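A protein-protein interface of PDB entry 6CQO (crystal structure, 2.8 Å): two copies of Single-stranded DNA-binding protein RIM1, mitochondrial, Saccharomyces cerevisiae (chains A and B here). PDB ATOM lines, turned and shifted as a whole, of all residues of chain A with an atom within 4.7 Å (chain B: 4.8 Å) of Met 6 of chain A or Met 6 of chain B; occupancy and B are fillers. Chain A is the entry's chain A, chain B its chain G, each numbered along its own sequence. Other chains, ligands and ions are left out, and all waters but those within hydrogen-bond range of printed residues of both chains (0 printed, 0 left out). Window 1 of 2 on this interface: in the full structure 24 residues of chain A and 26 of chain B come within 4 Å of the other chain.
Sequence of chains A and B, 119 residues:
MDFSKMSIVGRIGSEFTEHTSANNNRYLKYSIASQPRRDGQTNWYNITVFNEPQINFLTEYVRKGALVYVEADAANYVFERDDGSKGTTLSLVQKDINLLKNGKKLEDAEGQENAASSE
The backbone carbonyl oxygen (O) of Ser 4 of chain A lies within hydrogen-bond range of the backbone NH (N) of Ala 74 of chain A (2.5 Å). The backbone carbonyl oxygen (O) of Ala 72 of chain A sits at hydrogen-bond distance from the backbone NH (N) of Met 6 of chain A, 2.7 Å away. O of Ser 4 of chain B sits at hydrogen-bond distance from N of Ala 74 of chain B. The backbone carbonyl oxygen (O) of Ala 72 of chain B lies within hydrogen-bond range of the backbone NH (N) of Met 6 of chain B (2.7 Å).
Ser 4 of chain A touches Tyr 45 of chain B, and with the chains exchanged Tyr 45 of chain A touches Ser 4 of chain B. Lys 5 of chain A touches Met 6 of chain B, and with the chains exchanged Met 6 of chain A touches Lys 5 of chain B. Met 6 of chain A touches Ala 74 of chain B, and with the chains exchanged Ala 74 of chain A touches Met 6 of chain B. Tyr 45 of chain A touches Ala 74 of chain B, and with the chains exchanged Ala 74 of chain A touches Tyr 45 of chain B. 11 positions are printed for both chains.
Of chain B, only Lys 5, Met 6 and Ala 74 come within 4 Å of Met 6 of chain A. Of chain A, only Lys 5 (3.5 Å), Met 6 (3.6 Å) and Ala 74 (3.8 Å) come within 4 Å of Met 6 of chain B. Of the printed residues of chain B, Ser 4 of chain A touches Ser 7 and Tyr 45. Of the printed residues of chain A, Lys 5 of chain B touches Met 6 and Ser 7. Printed residues of chain A within 4 Å of Ala 74 of chain B: Met 6 and Tyr 45. Printed residues of chain A within 4 Å of Ser 7 of chain B: Ser 4 and Lys 5. Printed residues of chain A within 4 Å of Tyr 45 of chain B: Ser 4 and Ala 74. Ile 8 of chain B touches none of the printed residues of chain A. Leu 92 of chain B touches none of the printed residues of chain A. The nearest residue of chain B that does not touch Met 6 of chain A is Ser 4 of chain B (4.5 Å). The nearest printed residue of chain A that does not touch Lys 5 of chain B is Lys 5 of chain A (4.1 Å).
Of the 12 printed residues of chain B, 6 touch a printed residue of chain A. Printed residues of chain B that touch a printed residue of chain A: Ser 4, Lys 5, Met 6, Ser 7, Tyr 45 and Ala 74. Of the 11 printed residues of chain A, 6 touch a printed residue of chain B. Among the printed residues, 13 pairs touch across the chains. Among the printed residues, no Asp or Glu carboxylate lies within 4 Å of a Lys or Arg side-chain nitrogen of the other chain.
The side-chain hydroxyl of Tyr 45 of chain B sits at hydrogen-bond distance from the side-chain hydroxyl of Ser 4 of chain A (2.7 Å). The backbone carbonyl oxygen (O) of Lys 5 of chain A lies within hydrogen-bond range of the backbone NH (N) of Ser 7 of chain B. The backbone NH (N) of Ser 7 of chain A lies within hydrogen-bond range of the backbone carbonyl oxygen (O) of Lys 5 of chain B, at 3.1 Å. The side-chain hydroxyl (OH) of Tyr 45 of chain A sits at hydrogen-bond distance from the side-chain hydroxyl (OG) of Ser 4 of chain B (2.9 Å). OH of Tyr 45 of chain A is in hydrogen-bond range of O of Ala 74 of chain B. OH of Tyr 45 of chain B sits at hydrogen-bond distance from O of Ala 74 of chain A, 2.9 Å away.
Ser 7 of chain B touches Ser 4 of chain A. O of Lys 5 of chain A touches CA of Met 6 of chain B, at 3.5 Å. Met 6 of chain A touches Lys 5 of chain B. Met 6 of chain A touches Met 6 of chain B (CE to CE, 3.6 Å). Ala 74 of chain B touches Met 6 of chain A (CB to CE, 3.6 Å). Ser 7 of chain A touches Ser 4 of chain B. Ala 74 of chain A touches Met 6 of chain B.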
ATOM      1  N   SER A   4     -16.173   4.064  26.961  1.00  0.00           N
ATOM      2  CA  SER A   4     -17.435   4.433  26.326  1.00  0.00           C
ATOM      3  C   SER A   4     -17.586   3.572  25.081  1.00  0.00           C
ATOM      4  O   SER A   4     -16.898   3.797  24.080  1.00  0.00           O
ATOM      5  CB  SER A   4     -17.476   5.921  25.979  1.00  0.00           C
ATOM      6  OG  SER A   4     -16.403   6.277  25.125  1.00  0.00           O
ATOM      7  N   LYS A   5     -18.473   2.584  25.148  1.00  0.00           N
ATOM      8  CA  LYS A   5     -18.690   1.641  24.064  1.00  0.00           C
ATOM      9  C   LYS A   5     -20.133   1.738  23.589  1.00  0.00           C
ATOM     10  O   LYS A   5     -21.028   2.119  24.350  1.00  0.00           O
ATOM     11  CB  LYS A   5     -18.370   0.209  24.517  1.00  0.00           C
ATOM     12  CG  LYS A   5     -18.032  -0.751  23.393  1.00  0.00           C
ATOM     13  CD  LYS A   5     -17.490  -2.061  23.941  1.00  0.00           C
ATOM     14  CE  LYS A   5     -17.012  -2.971  22.822  1.00  0.00           C
ATOM     15  NZ  LYS A   5     -16.418  -4.229  23.347  1.00  0.00           N
ATOM     16  N   MET A   6     -20.355   1.400  22.323  1.00  0.00           N
ATOM     17  CA  MET A   6     -21.695   1.472  21.754  1.00  0.00           C
ATOM     18  C   MET A   6     -22.029   0.274  20.870  1.00  0.00           C
ATOM     19  O   MET A   6     -21.226  -0.139  20.033  1.00  0.00           O
ATOM     20  CB  MET A   6     -21.866   2.764  20.951  1.00  0.00           C
ATOM     21  CG  MET A   6     -23.224   2.888  20.276  1.00  0.00           C
ATOM     22  SD  MET A   6     -23.526   4.619  19.438  1.00  0.00           S
ATOM     23  CE  MET A   6     -23.228   5.752  20.985  1.00  0.00           C
ATOM     24  N   SER A   7     -23.221  -0.281  21.073  1.00  0.00           N
ATOM     25  CA  SER A   7     -23.766  -1.326  20.217  1.00  0.00           C
ATOM     26  C   SER A   7     -24.787  -0.704  19.274  1.00  0.00           C
ATOM     27  O   SER A   7     -25.640   0.076  19.707  1.00  0.00           O
ATOM     28  CB  SER A   7     -24.412  -2.436  21.048  1.00  0.00           C
ATOM     29  OG  SER A   7     -23.460  -3.073  21.884  1.00  0.00           O
ATOM     30  N   ILE A   8     -24.694  -1.046  17.990  1.00  0.00           N
ATOM     31  CA  ILE A   8     -25.534  -0.454  16.954  1.00  0.00           C
ATOM     32  C   ILE A   8     -26.111  -1.566  16.090  1.00  0.00           C
ATOM     33  O   ILE A   8     -25.375  -2.445  15.629  1.00  0.00           O
ATOM     34  CB  ILE A   8     -24.750   0.546  16.083  1.00  0.00           C
ATOM     35  CG1 ILE A   8     -24.273   1.737  16.916  1.00  0.00           C
ATOM     36  CG2 ILE A   8     -25.602   1.025  14.919  1.00  0.00           C
ATOM     37  CD1 ILE A   8     -23.486   2.758  16.123  1.00  0.00           C
ATOM     38  N   TYR A  45     -24.739   6.975  11.976  1.00  0.00           N
ATOM     39  CA  TYR A  45     -23.467   6.897  12.680  1.00  0.00           C
ATOM     40  C   TYR A  45     -22.353   6.601  11.688  1.00  0.00           C
ATOM     41  O   TYR A  45     -22.484   5.702  10.853  1.00  0.00           O
ATOM     42  CB  TYR A  45     -23.503   5.820  13.770  1.00  0.00           C
ATOM     43  CG  TYR A  45     -24.540   6.067  14.844  1.00  0.00           C
ATOM     44  CD1 TYR A  45     -24.277   6.920  15.907  1.00  0.00           C
ATOM     45  CD2 TYR A  45     -25.782   5.448  14.794  1.00  0.00           C
ATOM     46  CE1 TYR A  45     -25.221   7.149  16.891  1.00  0.00           C
ATOM     47  CE2 TYR A  45     -26.734   5.672  15.773  1.00  0.00           C
ATOM     48  CZ  TYR A  45     -26.446   6.524  16.818  1.00  0.00           C
ATOM     49  OH  TYR A  45     -27.388   6.751  17.794  1.00  0.00           O
ATOM     50  N   VAL A  70     -23.199  -3.905  15.148  1.00  0.00           N
ATOM     51  CA  VAL A  70     -21.842  -3.387  15.274  1.00  0.00           C
ATOM     52  C   VAL A  70     -21.595  -2.986  16.721  1.00  0.00           C
ATOM     53  O   VAL A  70     -22.426  -2.303  17.333  1.00  0.00           O
ATOM     54  CB  VAL A  70     -21.606  -2.195  14.327  1.00  0.00           C
ATOM     55  CG1 VAL A  70     -20.267  -1.533  14.619  1.00  0.00           C
ATOM     56  CG2 VAL A  70     -21.670  -2.653  12.881  1.00  0.00           C
ATOM     57  N   GLU A  71     -20.460  -3.418  17.263  1.00  0.00           N
ATOM     58  CA  GLU A  71     -19.961  -2.967  18.554  1.00  0.00           C
ATOM     59  C   GLU A  71     -18.748  -2.079  18.315  1.00  0.00           C
ATOM     60  O   GLU A  71     -17.823  -2.470  17.594  1.00  0.00           O
ATOM     61  CB  GLU A  71     -19.591  -4.154  19.446  1.00  0.00           C
ATOM     62  CG  GLU A  71     -20.775  -5.021  19.853  1.00  0.00           C
ATOM     63  CD  GLU A  71     -20.350  -6.337  20.478  1.00  0.00           C
ATOM     64  OE1 GLU A  71     -19.313  -6.891  20.055  1.00  0.00           O
ATOM     65  OE2 GLU A  71     -21.051  -6.817  21.394  1.00  0.00           O
ATOM     66  N   ALA A  72     -18.754  -0.887  18.909  1.00  0.00           N
ATOM     67  CA  ALA A  72     -17.719   0.099  18.635  1.00  0.00           C
ATOM     68  C   ALA A  72     -17.352   0.857  19.901  1.00  0.00           C
ATOM     69  O   ALA A  72     -18.211   1.134  20.741  1.00  0.00           O
ATOM     70  CB  ALA A  72     -18.172   1.089  17.554  1.00  0.00           C
ATOM     71  N   ALA A  74     -16.503   4.255  21.607  1.00  0.00           N
ATOM     72  CA  ALA A  74     -16.914   5.622  21.332  1.00  0.00           C
ATOM     73  C   ALA A  74     -15.933   6.613  21.943  1.00  0.00           C
ATOM     74  O   ALA A  74     -15.481   6.438  23.079  1.00  0.00           O
ATOM     75  CB  ALA A  74     -18.322   5.882  21.871  1.00  0.00           C
ATOM     76  N   LEU A  92     -16.477   6.419  16.284  1.00  0.00           N
ATOM     77  CA  LEU A  92     -16.919   5.049  16.546  1.00  0.00           C
ATOM     78  C   LEU A  92     -15.966   4.095  15.831  1.00  0.00           C
ATOM     79  O   LEU A  92     -16.153   3.781  14.653  1.00  0.00           O
ATOM     80  CB  LEU A  92     -18.363   4.850  16.094  1.00  0.00           C
ATOM     81  CG  LEU A  92     -19.387   5.800  16.713  1.00  0.00           C
ATOM     82  CD1 LEU A  92     -20.773   5.522  16.164  1.00  0.00           C
ATOM     83  CD2 LEU A  92     -19.373   5.684  18.227  1.00  0.00           C
ATOM     84  N   SER B   4     -29.361   1.829  19.378  1.00  0.00           N
ATOM     85  CA  SER B   4     -28.021   2.397  19.536  1.00  0.00           C
ATOM     86  C   SER B   4     -27.812   2.661  21.029  1.00  0.00           C
ATOM     87  O   SER B   4     -28.049   3.769  21.517  1.00  0.00           O
ATOM     88  CB  SER B   4     -27.849   3.661  18.706  1.00  0.00           C
ATOM     89  OG  SER B   4     -28.918   4.563  18.921  1.00  0.00           O
ATOM     90  N   LYS B   5     -27.371   1.628  21.743  1.00  0.00           N
ATOM     91  CA  LYS B   5     -27.150   1.707  23.180  1.00  0.00           C
ATOM     92  C   LYS B   5     -25.722   2.147  23.474  1.00  0.00           C
ATOM     93  O   LYS B   5     -24.775   1.702  22.821  1.00  0.00           O
ATOM     94  CB  LYS B   5     -27.416   0.355  23.842  1.00  0.00           C
ATOM     95  CG  LYS B   5     -28.784  -0.237  23.551  1.00  0.00           C
ATOM     96  CD  LYS B   5     -29.884   0.515  24.274  1.00  0.00           C
ATOM     97  CE  LYS B   5     -31.232  -0.159  24.069  1.00  0.00           C
ATOM     98  NZ  LYS B   5     -32.319   0.515  24.831  1.00  0.00           N
ATOM     99  N   MET B   6     -25.575   3.015  24.469  1.00  0.00           N
ATOM    100  CA  MET B   6     -24.258   3.475  24.892  1.00  0.00           C
ATOM    101  C   MET B   6     -24.011   3.153  26.363  1.00  0.00           C
ATOM    102  O   MET B   6     -24.866   3.405  27.214  1.00  0.00           O
ATOM    103  CB  MET B   6     -24.111   4.979  24.649  1.00  0.00           C
ATOM    104  CG  MET B   6     -22.870   5.586  25.285  1.00  0.00           C
ATOM    105  SD  MET B   6     -21.388   5.897  24.053  1.00  0.00           S
ATOM    106  CE  MET B   6     -21.783   7.744  23.574  1.00  0.00           C
ATOM    107  N   SER B   7     -22.841   2.588  26.654  1.00  0.00           N
ATOM    108  CA  SER B   7     -22.427   2.270  28.015  1.00  0.00           C
ATOM    109  C   SER B   7     -21.197   3.100  28.350  1.00  0.00           C
ATOM    110  O   SER B   7     -20.185   3.024  27.645  1.00  0.00           O
ATOM    111  CB  SER B   7     -22.131   0.777  28.169  1.00  0.00           C
ATOM    112  OG  SER B   7     -23.297   0.001  27.954  1.00  0.00           O
ATOM    113  N   ILE B   8     -21.285   3.887  29.420  1.00  0.00           N
ATOM    114  CA  ILE B   8     -20.233   4.823  29.800  1.00  0.00           C
ATOM    115  C   ILE B   8     -19.867   4.592  31.258  1.00  0.00           C
ATOM    116  O   ILE B   8     -20.752   4.470  32.113  1.00  0.00           O
ATOM    117  CB  ILE B   8     -20.666   6.287  29.590  1.00  0.00           C
ATOM    118  CG1 ILE B   8     -21.104   6.517  28.146  1.00  0.00           C
ATOM    119  CG2 ILE B   8     -19.534   7.237  29.952  1.00  0.00           C
ATOM    120  CD1 ILE B   8     -21.683   7.894  27.896  1.00  0.00           C
ATOM    121  N   TYR B  45     -19.338  13.540  27.575  1.00  0.00           N
ATOM    122  CA  TYR B  45     -20.646  13.163  27.060  1.00  0.00           C
ATOM    123  C   TYR B  45     -21.725  13.892  27.840  1.00  0.00           C
ATOM    124  O   TYR B  45     -21.768  13.813  29.072  1.00  0.00           O
ATOM    125  CB  TYR B  45     -20.864  11.648  27.149  1.00  0.00           C
ATOM    126  CG  TYR B  45     -19.887  10.835  26.330  1.00  0.00           C
ATOM    127  CD1 TYR B  45     -20.012  10.749  24.950  1.00  0.00           C
ATOM    128  CD2 TYR B  45     -18.846  10.145  26.939  1.00  0.00           C
ATOM    129  CE1 TYR B  45     -19.123  10.006  24.199  1.00  0.00           C
ATOM    130  CE2 TYR B  45     -17.954   9.400  26.195  1.00  0.00           C
ATOM    131  CZ  TYR B  45     -18.097   9.332  24.825  1.00  0.00           C
ATOM    132  OH  TYR B  45     -17.211   8.588  24.076  1.00  0.00           O
ATOM    133  N   VAL B  70     -23.263   4.378  33.327  1.00  0.00           N
ATOM    134  CA  VAL B  70     -24.515   4.866  32.766  1.00  0.00           C
ATOM    135  C   VAL B  70     -24.826   4.075  31.503  1.00  0.00           C
ATOM    136  O   VAL B  70     -23.949   3.876  30.653  1.00  0.00           O
ATOM    137  CB  VAL B  70     -24.441   6.374  32.466  1.00  0.00           C
ATOM    138  CG1 VAL B  70     -25.703   6.845  31.760  1.00  0.00           C
ATOM    139  CG2 VAL B  70     -24.215   7.160  33.746  1.00  0.00           C
ATOM    140  N   GLU B  71     -26.070   3.619  31.388  1.00  0.00           N
ATOM    141  CA  GLU B  71     -26.605   3.073  30.148  1.00  0.00           C
ATOM    142  C   GLU B  71     -27.545   4.110  29.553  1.00  0.00           C
ATOM    143  O   GLU B  71     -28.512   4.521  30.203  1.00  0.00           O
ATOM    144  CB  GLU B  71     -27.343   1.756  30.384  1.00  0.00           C
ATOM    145  CG  GLU B  71     -26.455   0.597  30.790  1.00  0.00           C
ATOM    146  CD  GLU B  71     -27.159  -0.739  30.649  1.00  0.00           C
ATOM    147  OE1 GLU B  71     -26.685  -1.577  29.852  1.00  0.00           O
ATOM    148  OE2 GLU B  71     -28.193  -0.944  31.320  1.00  0.00           O
ATOM    149  N   ALA B  72     -27.261   4.534  28.325  1.00  0.00           N
ATOM    150  CA  ALA B  72     -28.045   5.579  27.685  1.00  0.00           C
ATOM    151  C   ALA B  72     -28.331   5.205  26.241  1.00  0.00           C
ATOM    152  O   ALA B  72     -27.491   4.601  25.568  1.00  0.00           O
ATOM    153  CB  ALA B  72     -27.322   6.930  27.739  1.00  0.00           C
ATOM    154  N   ALA B  74     -28.705   6.265  22.422  1.00  0.00           N
ATOM    155  CA  ALA B  74     -28.030   7.252  21.591  1.00  0.00           C
ATOM    156  C   ALA B  74     -28.871   7.566  20.363  1.00  0.00           C
ATOM    157  O   ALA B  74     -29.389   6.656  19.708  1.00  0.00           O
ATOM    158  CB  ALA B  74     -26.646   6.757  21.169  1.00  0.00           C
ATOM    159  N   LEU B  90     -25.437  14.631  18.654  1.00  0.00           N
ATOM    160  CA  LEU B  90     -25.473  13.443  19.494  1.00  0.00           C
ATOM    161  C   LEU B  90     -26.368  13.684  20.703  1.00  0.00           C
ATOM    162  O   LEU B  90     -26.291  14.739  21.341  1.00  0.00           O
ATOM    163  CB  LEU B  90     -24.063  13.061  19.946  1.00  0.00           C
ATOM    164  CG  LEU B  90     -23.947  11.821  20.834  1.00  0.00           C
ATOM    165  CD1 LEU B  90     -24.469  10.591  20.108  1.00  0.00           C
ATOM    166  CD2 LEU B  90     -22.509  11.615  21.279  1.00  0.00           C
ATOM    167  N   LEU B  92     -27.855  11.612  24.276  1.00  0.00           N
ATOM    168  CA  LEU B  92     -27.701  10.469  25.172  1.00  0.00           C
ATOM    169  C   LEU B  92     -28.735  10.582  26.285  1.00  0.00           C
ATOM    170  O   LEU B  92     -28.587  11.404  27.194  1.00  0.00           O
ATOM    171  CB  LEU B  92     -26.287  10.407  25.749  1.00  0.00           C
ATOM    172  CG  LEU B  92     -25.153  10.195  24.746  1.00  0.00           C
ATOM    173  CD1 LEU B  92     -23.805  10.247  25.445  1.00  0.00           C
ATOM    174  CD2 LEU B  92     -25.331   8.877  24.013  1.00  0.00           C
